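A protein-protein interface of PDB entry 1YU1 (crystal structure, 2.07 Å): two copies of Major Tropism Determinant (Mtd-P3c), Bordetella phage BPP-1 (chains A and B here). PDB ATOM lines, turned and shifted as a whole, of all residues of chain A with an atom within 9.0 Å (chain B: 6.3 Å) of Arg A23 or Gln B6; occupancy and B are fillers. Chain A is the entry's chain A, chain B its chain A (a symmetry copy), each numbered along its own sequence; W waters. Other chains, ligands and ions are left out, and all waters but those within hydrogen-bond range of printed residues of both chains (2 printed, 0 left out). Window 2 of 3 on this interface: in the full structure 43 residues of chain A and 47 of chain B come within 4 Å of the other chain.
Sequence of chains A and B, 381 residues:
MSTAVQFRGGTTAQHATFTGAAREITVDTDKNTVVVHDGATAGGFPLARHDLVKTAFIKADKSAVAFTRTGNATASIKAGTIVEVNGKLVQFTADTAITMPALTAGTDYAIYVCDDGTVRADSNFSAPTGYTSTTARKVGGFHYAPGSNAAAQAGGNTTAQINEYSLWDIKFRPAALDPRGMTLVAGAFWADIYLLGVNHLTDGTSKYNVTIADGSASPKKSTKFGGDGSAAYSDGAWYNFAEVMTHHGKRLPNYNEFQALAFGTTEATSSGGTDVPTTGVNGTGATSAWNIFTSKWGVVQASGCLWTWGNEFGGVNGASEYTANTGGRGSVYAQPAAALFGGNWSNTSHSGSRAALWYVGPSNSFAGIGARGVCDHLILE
The side-chain amide oxygen (OE1) of Gln B6 sits close to the backbone carbonyl oxygen (O) of Ala A22 (3.0 Å).
NH2 of Arg A23 sits at hydrogen-bond distance from OE1 of Gln B6.
The backbone carbonyl oxygen (O) of Arg A23 lies within hydrogen-bond range of the backbone NH (N) of Phe B7.
N of Ala A21 lies within hydrogen-bond range of OE1 of Glu A24, 2.9 Å away.
O of His A37 is in hydrogen-bond range of N of Arg A23, 3.1 Å away.
The backbone carbonyl oxygen of Glu A24 lies within hydrogen-bond range of the backbone NH of His A37 (3.0 Å).
The backbone carbonyl oxygen (O) of Val A36 lies within hydrogen-bond range of the backbone NH (N) of Phe A45 (2.8 Å).
The backbone carbonyl oxygen (O) of Arg B8 sits at hydrogen-bond distance from the backbone NH (N) of Val B27 (3.0 Å).
The backbone NH (N) of Gly B10 sits at hydrogen-bond distance from the backbone carbonyl oxygen (O) of Val B27 (3.2 Å).
Among the printed residues, pairs that only touch across the chains: Phe A7 with Phe B7 (3.4 Å), Ala A21 with Gln B6 (3.8 Å), Arg A23 with Gly B9 (3.8 Å), Glu A24 with Val B5 (3.5 Å), Ile A25 with Phe B7 (3.7 Å), Ile A25 with Val B27 (3.9 Å) and Val A36 with Val B27 (3.9 Å).
Of the printed residues of chain B, Ala A22 touches Gln B6.
Of chain B, only Gln B6 (3.2 Å), Phe B7 (2.9 Å) and Gly B9 (3.8 Å) come within 4 Å of Arg A23.
Of the printed residues of chain B, Ile A25 touches Phe B7 and Val B27.
Printed residues of chain B within 4 Å of Val A36: Val B27.
Val B5 touches just one residue of chain A: Glu A24.
Gln B6 touches just these residues of chain A: Ala A21 (3.8 Å), Ala A22 (3.0 Å) and Arg A23 (3.2 Å).
The nearest residue of chain B that does not touch Arg A23 is Thr B29 (4.02 Å).
Of the 16 printed residues of chain A, 7 touch a printed residue of chain B.
Printed residues of chain A that touch a printed residue of chain B: Phe A7, Ala A21, Ala A22, Arg A23, Glu A24, Ile A25 and Val A36.
Hydrophobic or aromatic side chains of chain B that line the printed part of chain A: Phe B7 and Val B27.
Among the printed residues, 10 pairs touch across the chains.
Among the printed residues, no Asp or Glu carboxylate lies within 4 Å of a Lys or Arg side-chain nitrogen of the other chain.
Phe A7 touches its own counterpart, Phe B7.
1 position is printed for both chains.
Water W2 lies within hydrogen-bond range of the backbone carbonyl oxygen of Val B5 (2.6 Å) and the backbone NH of Ile A25 (3.2 Å).
Water W1 lies within hydrogen-bond range of the backbone carbonyl oxygen of Phe B7 (2.9 Å), the guanidinium group of Arg A23 (3.2 Å) and the backbone carbonyl oxygen of Gln B6 (3.3 Å).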
ATOM      1  N   PHE A   7      23.641  20.152  12.113  1.00  0.00           N
ATOM      2  CA  PHE A   7      22.217  20.010  12.371  1.00  0.00           C
ATOM      3  C   PHE A   7      21.605  18.936  11.501  1.00  0.00           C
ATOM      4  O   PHE A   7      22.187  18.533  10.498  1.00  0.00           O
ATOM      5  CB  PHE A   7      21.515  21.338  12.127  1.00  0.00           C
ATOM      6  CG  PHE A   7      21.573  22.248  13.297  1.00  0.00           C
ATOM      7  CD1 PHE A   7      20.477  22.386  14.122  1.00  0.00           C
ATOM      8  CD2 PHE A   7      22.742  22.929  13.603  1.00  0.00           C
ATOM      9  CE1 PHE A   7      20.526  23.205  15.216  1.00  0.00           C
ATOM     10  CE2 PHE A   7      22.802  23.754  14.701  1.00  0.00           C
ATOM     11  CZ  PHE A   7      21.688  23.895  15.513  1.00  0.00           C
ATOM     12  N   GLY A  20       8.592  18.148  11.496  1.00  0.00           N
ATOM     13  CA  GLY A  20       9.435  18.186  12.681  1.00  0.00           C
ATOM     14  C   GLY A  20       8.653  18.637  13.899  1.00  0.00           C
ATOM     15  O   GLY A  20       7.567  19.193  13.769  1.00  0.00           O
ATOM     16  N   ALA A  21       9.207  18.386  15.081  1.00  0.00           N
ATOM     17  CA  ALA A  21       8.603  18.808  16.340  1.00  0.00           C
ATOM     18  C   ALA A  21       8.537  20.323  16.440  1.00  0.00           C
ATOM     19  O   ALA A  21       9.221  21.034  15.704  1.00  0.00           O
ATOM     20  CB  ALA A  21       9.401  18.245  17.511  1.00  0.00           C
ATOM     21  N   ALA A  22       7.712  20.815  17.356  1.00  0.00           N
ATOM     22  CA  ALA A  22       7.607  22.248  17.598  1.00  0.00           C
ATOM     23  C   ALA A  22       8.952  22.797  18.067  1.00  0.00           C
ATOM     24  O   ALA A  22       9.595  22.217  18.944  1.00  0.00           O
ATOM     25  CB  ALA A  22       6.519  22.542  18.623  1.00  0.00           C
ATOM     26  N   ARG A  23       9.368  23.907  17.457  1.00  0.00           N
ATOM     27  CA  ARG A  23      10.655  24.563  17.719  1.00  0.00           C
ATOM     28  C   ARG A  23      11.891  23.778  17.248  1.00  0.00           C
ATOM     29  O   ARG A  23      13.011  24.138  17.594  1.00  0.00           O
ATOM     30  CB  ARG A  23      10.788  24.952  19.199  1.00  0.00           C
ATOM     31  CG  ARG A  23       9.588  25.739  19.746  1.00  0.00           C
ATOM     32  CD  ARG A  23       9.606  25.982  21.258  1.00  0.00           C
ATOM     33  NE  ARG A  23       9.927  24.779  22.027  1.00  0.00           N
ATOM     34  CZ  ARG A  23       9.102  23.752  22.232  1.00  0.00           C
ATOM     35  NH1 ARG A  23       7.862  23.746  21.747  1.00  0.00           N
ATOM     36  NH2 ARG A  23       9.524  22.715  22.947  1.00  0.00           N
ATOM     37  N   GLU A  24      11.696  22.738  16.437  1.00  0.00           N
ATOM     38  CA  GLU A  24      12.813  22.027  15.816  1.00  0.00           C
ATOM     39  C   GLU A  24      13.283  22.808  14.589  1.00  0.00           C
ATOM     40  O   GLU A  24      12.467  23.353  13.842  1.00  0.00           O
ATOM     41  CB  GLU A  24      12.416  20.601  15.402  1.00  0.00           C
ATOM     42  CG  GLU A  24      13.560  19.795  14.788  1.00  0.00           C
ATOM     43  CD  GLU A  24      13.166  18.389  14.345  1.00  0.00           C
ATOM     44  OE1 GLU A  24      12.013  17.968  14.560  1.00  0.00           O
ATOM     45  OE2 GLU A  24      14.026  17.694  13.769  1.00  0.00           O
ATOM     46  N   ILE A  25      14.600  22.838  14.394  1.00  0.00           N
ATOM     47  CA  ILE A  25      15.234  23.551  13.290  1.00  0.00           C
ATOM     48  C   ILE A  25      16.062  22.581  12.449  1.00  0.00           C
ATOM     49  O   ILE A  25      17.014  21.982  12.947  1.00  0.00           O
ATOM     50  CB  ILE A  25      16.145  24.670  13.842  1.00  0.00           C
ATOM     51  CG1 ILE A  25      15.298  25.814  14.401  1.00  0.00           C
ATOM     52  CG2 ILE A  25      17.093  25.190  12.760  1.00  0.00           C
ATOM     53  CD1 ILE A  25      16.076  26.774  15.283  1.00  0.00           C
ATOM     54  N   THR A  26      15.699  22.436  11.178  1.00  0.00           N
ATOM     55  CA  THR A  26      16.450  21.606  10.244  1.00  0.00           C
ATOM     56  C   THR A  26      17.094  22.464   9.162  1.00  0.00           C
ATOM     57  O   THR A  26      16.856  23.675   9.093  1.00  0.00           O
ATOM     58  CB  THR A  26      15.539  20.539   9.609  1.00  0.00           C
ATOM     59  OG1 THR A  26      14.461  21.164   8.904  1.00  0.00           O
ATOM     60  CG2 THR A  26      14.851  19.697  10.686  1.00  0.00           C
ATOM     61  N   VAL A  34      17.683  27.494   6.630  1.00  0.00           N
ATOM     62  CA  VAL A  34      17.093  26.942   7.835  1.00  0.00           C
ATOM     63  C   VAL A  34      15.590  26.773   7.613  1.00  0.00           C
ATOM     64  O   VAL A  34      14.968  27.557   6.893  1.00  0.00           O
ATOM     65  CB  VAL A  34      17.392  27.876   9.040  1.00  0.00           C
ATOM     66  CG1 VAL A  34      16.407  27.680  10.185  1.00  0.00           C
ATOM     67  CG2 VAL A  34      18.823  27.665   9.518  1.00  0.00           C
ATOM     68  N   VAL A  35      15.021  25.741   8.230  1.00  0.00           N
ATOM     69  CA  VAL A  35      13.592  25.457   8.169  1.00  0.00           C
ATOM     70  C   VAL A  35      13.053  25.300   9.603  1.00  0.00           C
ATOM     71  O   VAL A  35      13.510  24.436  10.350  1.00  0.00           O
ATOM     72  CB  VAL A  35      13.319  24.189   7.336  1.00  0.00           C
ATOM     73  CG1 VAL A  35      11.835  23.910   7.228  1.00  0.00           C
ATOM     74  CG2 VAL A  35      13.921  24.329   5.943  1.00  0.00           C
ATOM     75  N   VAL A  36      12.094  26.150   9.972  1.00  0.00           N
ATOM     76  CA  VAL A  36      11.496  26.156  11.310  1.00  0.00           C
ATOM     77  C   VAL A  36      10.236  25.301  11.327  1.00  0.00           C
ATOM     78  O   VAL A  36       9.416  25.386  10.415  1.00  0.00           O
ATOM     79  CB  VAL A  36      11.129  27.593  11.750  1.00  0.00           C
ATOM     80  CG1 VAL A  36      10.413  27.594  13.104  1.00  0.00           C
ATOM     81  CG2 VAL A  36      12.373  28.462  11.803  1.00  0.00           C
ATOM     82  N   HIS A  37      10.074  24.489  12.368  1.00  0.00           N
ATOM     83  CA  HIS A  37       8.981  23.516  12.426  1.00  0.00           C
ATOM     84  C   HIS A  37       8.060  23.758  13.622  1.00  0.00           C
ATOM     85  O   HIS A  37       8.433  24.435  14.578  1.00  0.00           O
ATOM     86  CB  HIS A  37       9.551  22.094  12.430  1.00  0.00           C
ATOM     87  CG  HIS A  37      10.168  21.696  11.124  1.00  0.00           C
ATOM     88  ND1 HIS A  37      10.357  20.386  10.755  1.00  0.00           N
ATOM     89  CD2 HIS A  37      10.630  22.439  10.092  1.00  0.00           C
ATOM     90  CE1 HIS A  37      10.915  20.338   9.560  1.00  0.00           C
ATOM     91  NE2 HIS A  37      11.091  21.570   9.135  1.00  0.00           N
ATOM     92  N   ASP A  38       6.847  23.212  13.540  1.00  0.00           N
ATOM     93  CA  ASP A  38       5.781  23.494  14.513  1.00  0.00           C
ATOM     94  C   ASP A  38       5.045  22.259  15.075  1.00  0.00           C
ATOM     95  O   ASP A  38       4.186  22.404  15.939  1.00  0.00           O
ATOM     96  CB  ASP A  38       4.763  24.468  13.901  1.00  0.00           C
ATOM     97  CG  ASP A  38       3.925  23.838  12.795  1.00  0.00           C
ATOM     98  OD1 ASP A  38       4.346  22.805  12.239  1.00  0.00           O
ATOM     99  OD2 ASP A  38       2.837  24.318  12.405  1.00  0.00           O
ATOM    100  N   GLY A  39       5.370  21.066  14.579  1.00  0.00           N
ATOM    101  CA  GLY A  39       4.768  19.828  15.057  1.00  0.00           C
ATOM    102  C   GLY A  39       3.507  19.391  14.326  1.00  0.00           C
ATOM    103  O   GLY A  39       2.847  18.440  14.755  1.00  0.00           O
ATOM    104  N   ALA A  40       3.180  20.058  13.218  1.00  0.00           N
ATOM    105  CA  ALA A  40       1.926  19.817  12.496  1.00  0.00           C
ATOM    106  C   ALA A  40       2.025  20.051  10.981  1.00  0.00           C
ATOM    107  O   ALA A  40       1.524  19.250  10.188  1.00  0.00           O
ATOM    108  CB  ALA A  40       0.826  20.681  13.081  1.00  0.00           C
ATOM    109  N   PHE A  45       8.690  25.620   7.707  1.00  0.00           N
ATOM    110  CA  PHE A  45       8.612  27.026   7.339  1.00  0.00           C
ATOM    111  C   PHE A  45      10.015  27.518   6.976  1.00  0.00           C
ATOM    112  O   PHE A  45      10.752  28.005   7.837  1.00  0.00           O
ATOM    113  CB  PHE A  45       8.031  27.837   8.499  1.00  0.00           C
ATOM    114  CG  PHE A  45       6.638  27.420   8.894  1.00  0.00           C
ATOM    115  CD1 PHE A  45       5.531  27.957   8.254  1.00  0.00           C
ATOM    116  CD2 PHE A  45       6.432  26.487   9.906  1.00  0.00           C
ATOM    117  CE1 PHE A  45       4.242  27.578   8.613  1.00  0.00           C
ATOM    118  CE2 PHE A  45       5.151  26.104  10.269  1.00  0.00           C
ATOM    119  CZ  PHE A  45       4.050  26.653   9.624  1.00  0.00           C
ATOM    120  N   VAL B   5      15.227  17.266  18.695  1.00  0.00           N
ATOM    121  CA  VAL B   5      15.843  18.446  19.376  1.00  0.00           C
ATOM    122  C   VAL B   5      15.041  19.722  19.132  1.00  0.00           C
ATOM    123  O   VAL B   5      14.915  20.185  17.994  1.00  0.00           O
ATOM    124  CB  VAL B   5      17.287  18.700  18.908  1.00  0.00           C
ATOM    125  CG1 VAL B   5      17.898  19.883  19.669  1.00  0.00           C
ATOM    126  CG2 VAL B   5      18.135  17.455  19.083  1.00  0.00           C
ATOM    127  N   GLN B   6      14.524  20.295  20.215  1.00  0.00           N
ATOM    128  CA  GLN B   6      13.676  21.472  20.150  1.00  0.00           C
ATOM    129  C   GLN B   6      14.359  22.656  20.825  1.00  0.00           C
ATOM    130  O   GLN B   6      15.030  22.511  21.846  1.00  0.00           O
ATOM    131  CB  GLN B   6      12.330  21.170  20.804  1.00  0.00           C
ATOM    132  CG  GLN B   6      11.611  19.984  20.163  1.00  0.00           C
ATOM    133  CD  GLN B   6      10.440  19.489  20.983  1.00  0.00           C
ATOM    134  OE1 GLN B   6       9.413  20.156  21.067  1.00  0.00           O
ATOM    135  NE2 GLN B   6      10.591  18.317  21.591  1.00  0.00           N
ATOM    136  N   PHE B   7      14.174  23.834  20.247  1.00  0.00           N
ATOM    137  CA  PHE B   7      14.829  25.043  20.718  1.00  0.00           C
ATOM    138  C   PHE B   7      13.949  25.806  21.682  1.00  0.00           C
ATOM    139  O   PHE B   7      12.743  25.585  21.740  1.00  0.00           O
ATOM    140  CB  PHE B   7      15.190  25.929  19.534  1.00  0.00           C
ATOM    141  CG  PHE B   7      16.477  25.551  18.899  1.00  0.00           C
ATOM    142  CD1 PHE B   7      17.616  26.284  19.158  1.00  0.00           C
ATOM    143  CD2 PHE B   7      16.559  24.434  18.082  1.00  0.00           C
ATOM    144  CE1 PHE B   7      18.813  25.933  18.597  1.00  0.00           C
ATOM    145  CE2 PHE B   7      17.758  24.072  17.513  1.00  0.00           C
ATOM    146  CZ  PHE B   7      18.893  24.826  17.770  1.00  0.00           C
ATOM    147  N   ARG B   8      14.570  26.695  22.448  1.00  0.00           N
ATOM    148  CA  ARG B   8      13.834  27.607  23.307  1.00  0.00           C
ATOM    149  C   ARG B   8      12.965  28.484  22.416  1.00  0.00           C
ATOM    150  O   ARG B   8      13.422  28.967  21.382  1.00  0.00           O
ATOM    151  CB  ARG B   8      14.796  28.467  24.137  1.00  0.00           C
ATOM    152  CG  ARG B   8      14.145  29.676  24.805  1.00  0.00           C
ATOM    153  CD  ARG B   8      14.420  29.813  26.287  1.00  0.00           C
ATOM    154  NE  ARG B   8      15.587  30.650  26.553  1.00  0.00           N
ATOM    155  CZ  ARG B   8      15.746  31.411  27.634  1.00  0.00           C
ATOM    156  NH1 ARG B   8      14.811  31.464  28.582  1.00  0.00           N
ATOM    157  NH2 ARG B   8      16.852  32.132  27.774  1.00  0.00           N
ATOM    158  N   GLY B   9      11.712  28.670  22.815  1.00  0.00           N
ATOM    159  CA  GLY B   9      10.785  29.477  22.048  1.00  0.00           C
ATOM    160  C   GLY B   9       9.710  30.145  22.876  1.00  0.00           C
ATOM    161  O   GLY B   9       9.429  29.752  24.010  1.00  0.00           O
ATOM    162  N   GLY B  10       9.112  31.173  22.289  1.00  0.00           N
ATOM    163  CA  GLY B  10       8.011  31.894  22.901  1.00  0.00           C
ATOM    164  C   GLY B  10       7.207  32.646  21.862  1.00  0.00           C
ATOM    165  O   GLY B  10       7.616  32.762  20.703  1.00  0.00           O
ATOM    166  N   VAL B  27      13.032  30.695  18.969  1.00  0.00           N
ATOM    167  CA  VAL B  27      12.027  30.463  17.944  1.00  0.00           C
ATOM    168  C   VAL B  27      10.731  31.171  18.326  1.00  0.00           C
ATOM    169  O   VAL B  27      10.094  30.821  19.316  1.00  0.00           O
ATOM    170  CB  VAL B  27      11.763  28.953  17.748  1.00  0.00           C
ATOM    171  CG1 VAL B  27      10.560  28.710  16.833  1.00  0.00           C
ATOM    172  CG2 VAL B  27      13.001  28.269  17.183  1.00  0.00           C
ATOM    173  N   THR B  29       7.125  31.372  17.974  1.00  0.00           N
ATOM    174  CA  THR B  29       6.170  30.313  17.634  1.00  0.00           C
ATOM    175  C   THR B  29       4.895  30.834  16.976  1.00  0.00           C
ATOM    176  O   THR B  29       4.157  30.063  16.358  1.00  0.00           O
ATOM    177  CB  THR B  29       5.810  29.481  18.889  1.00  0.00           C
ATOM    178  OG1 THR B  29       5.323  30.335  19.933  1.00  0.00           O
ATOM    179  CG2 THR B  29       7.046  28.843  19.489  1.00  0.00           C
HETATM  180  O   HOH W   1      12.534  23.530  23.825  1.00  0.00           O
HETATM  181  O   HOH W   2      16.543  21.010  16.154  1.00  0.00           O
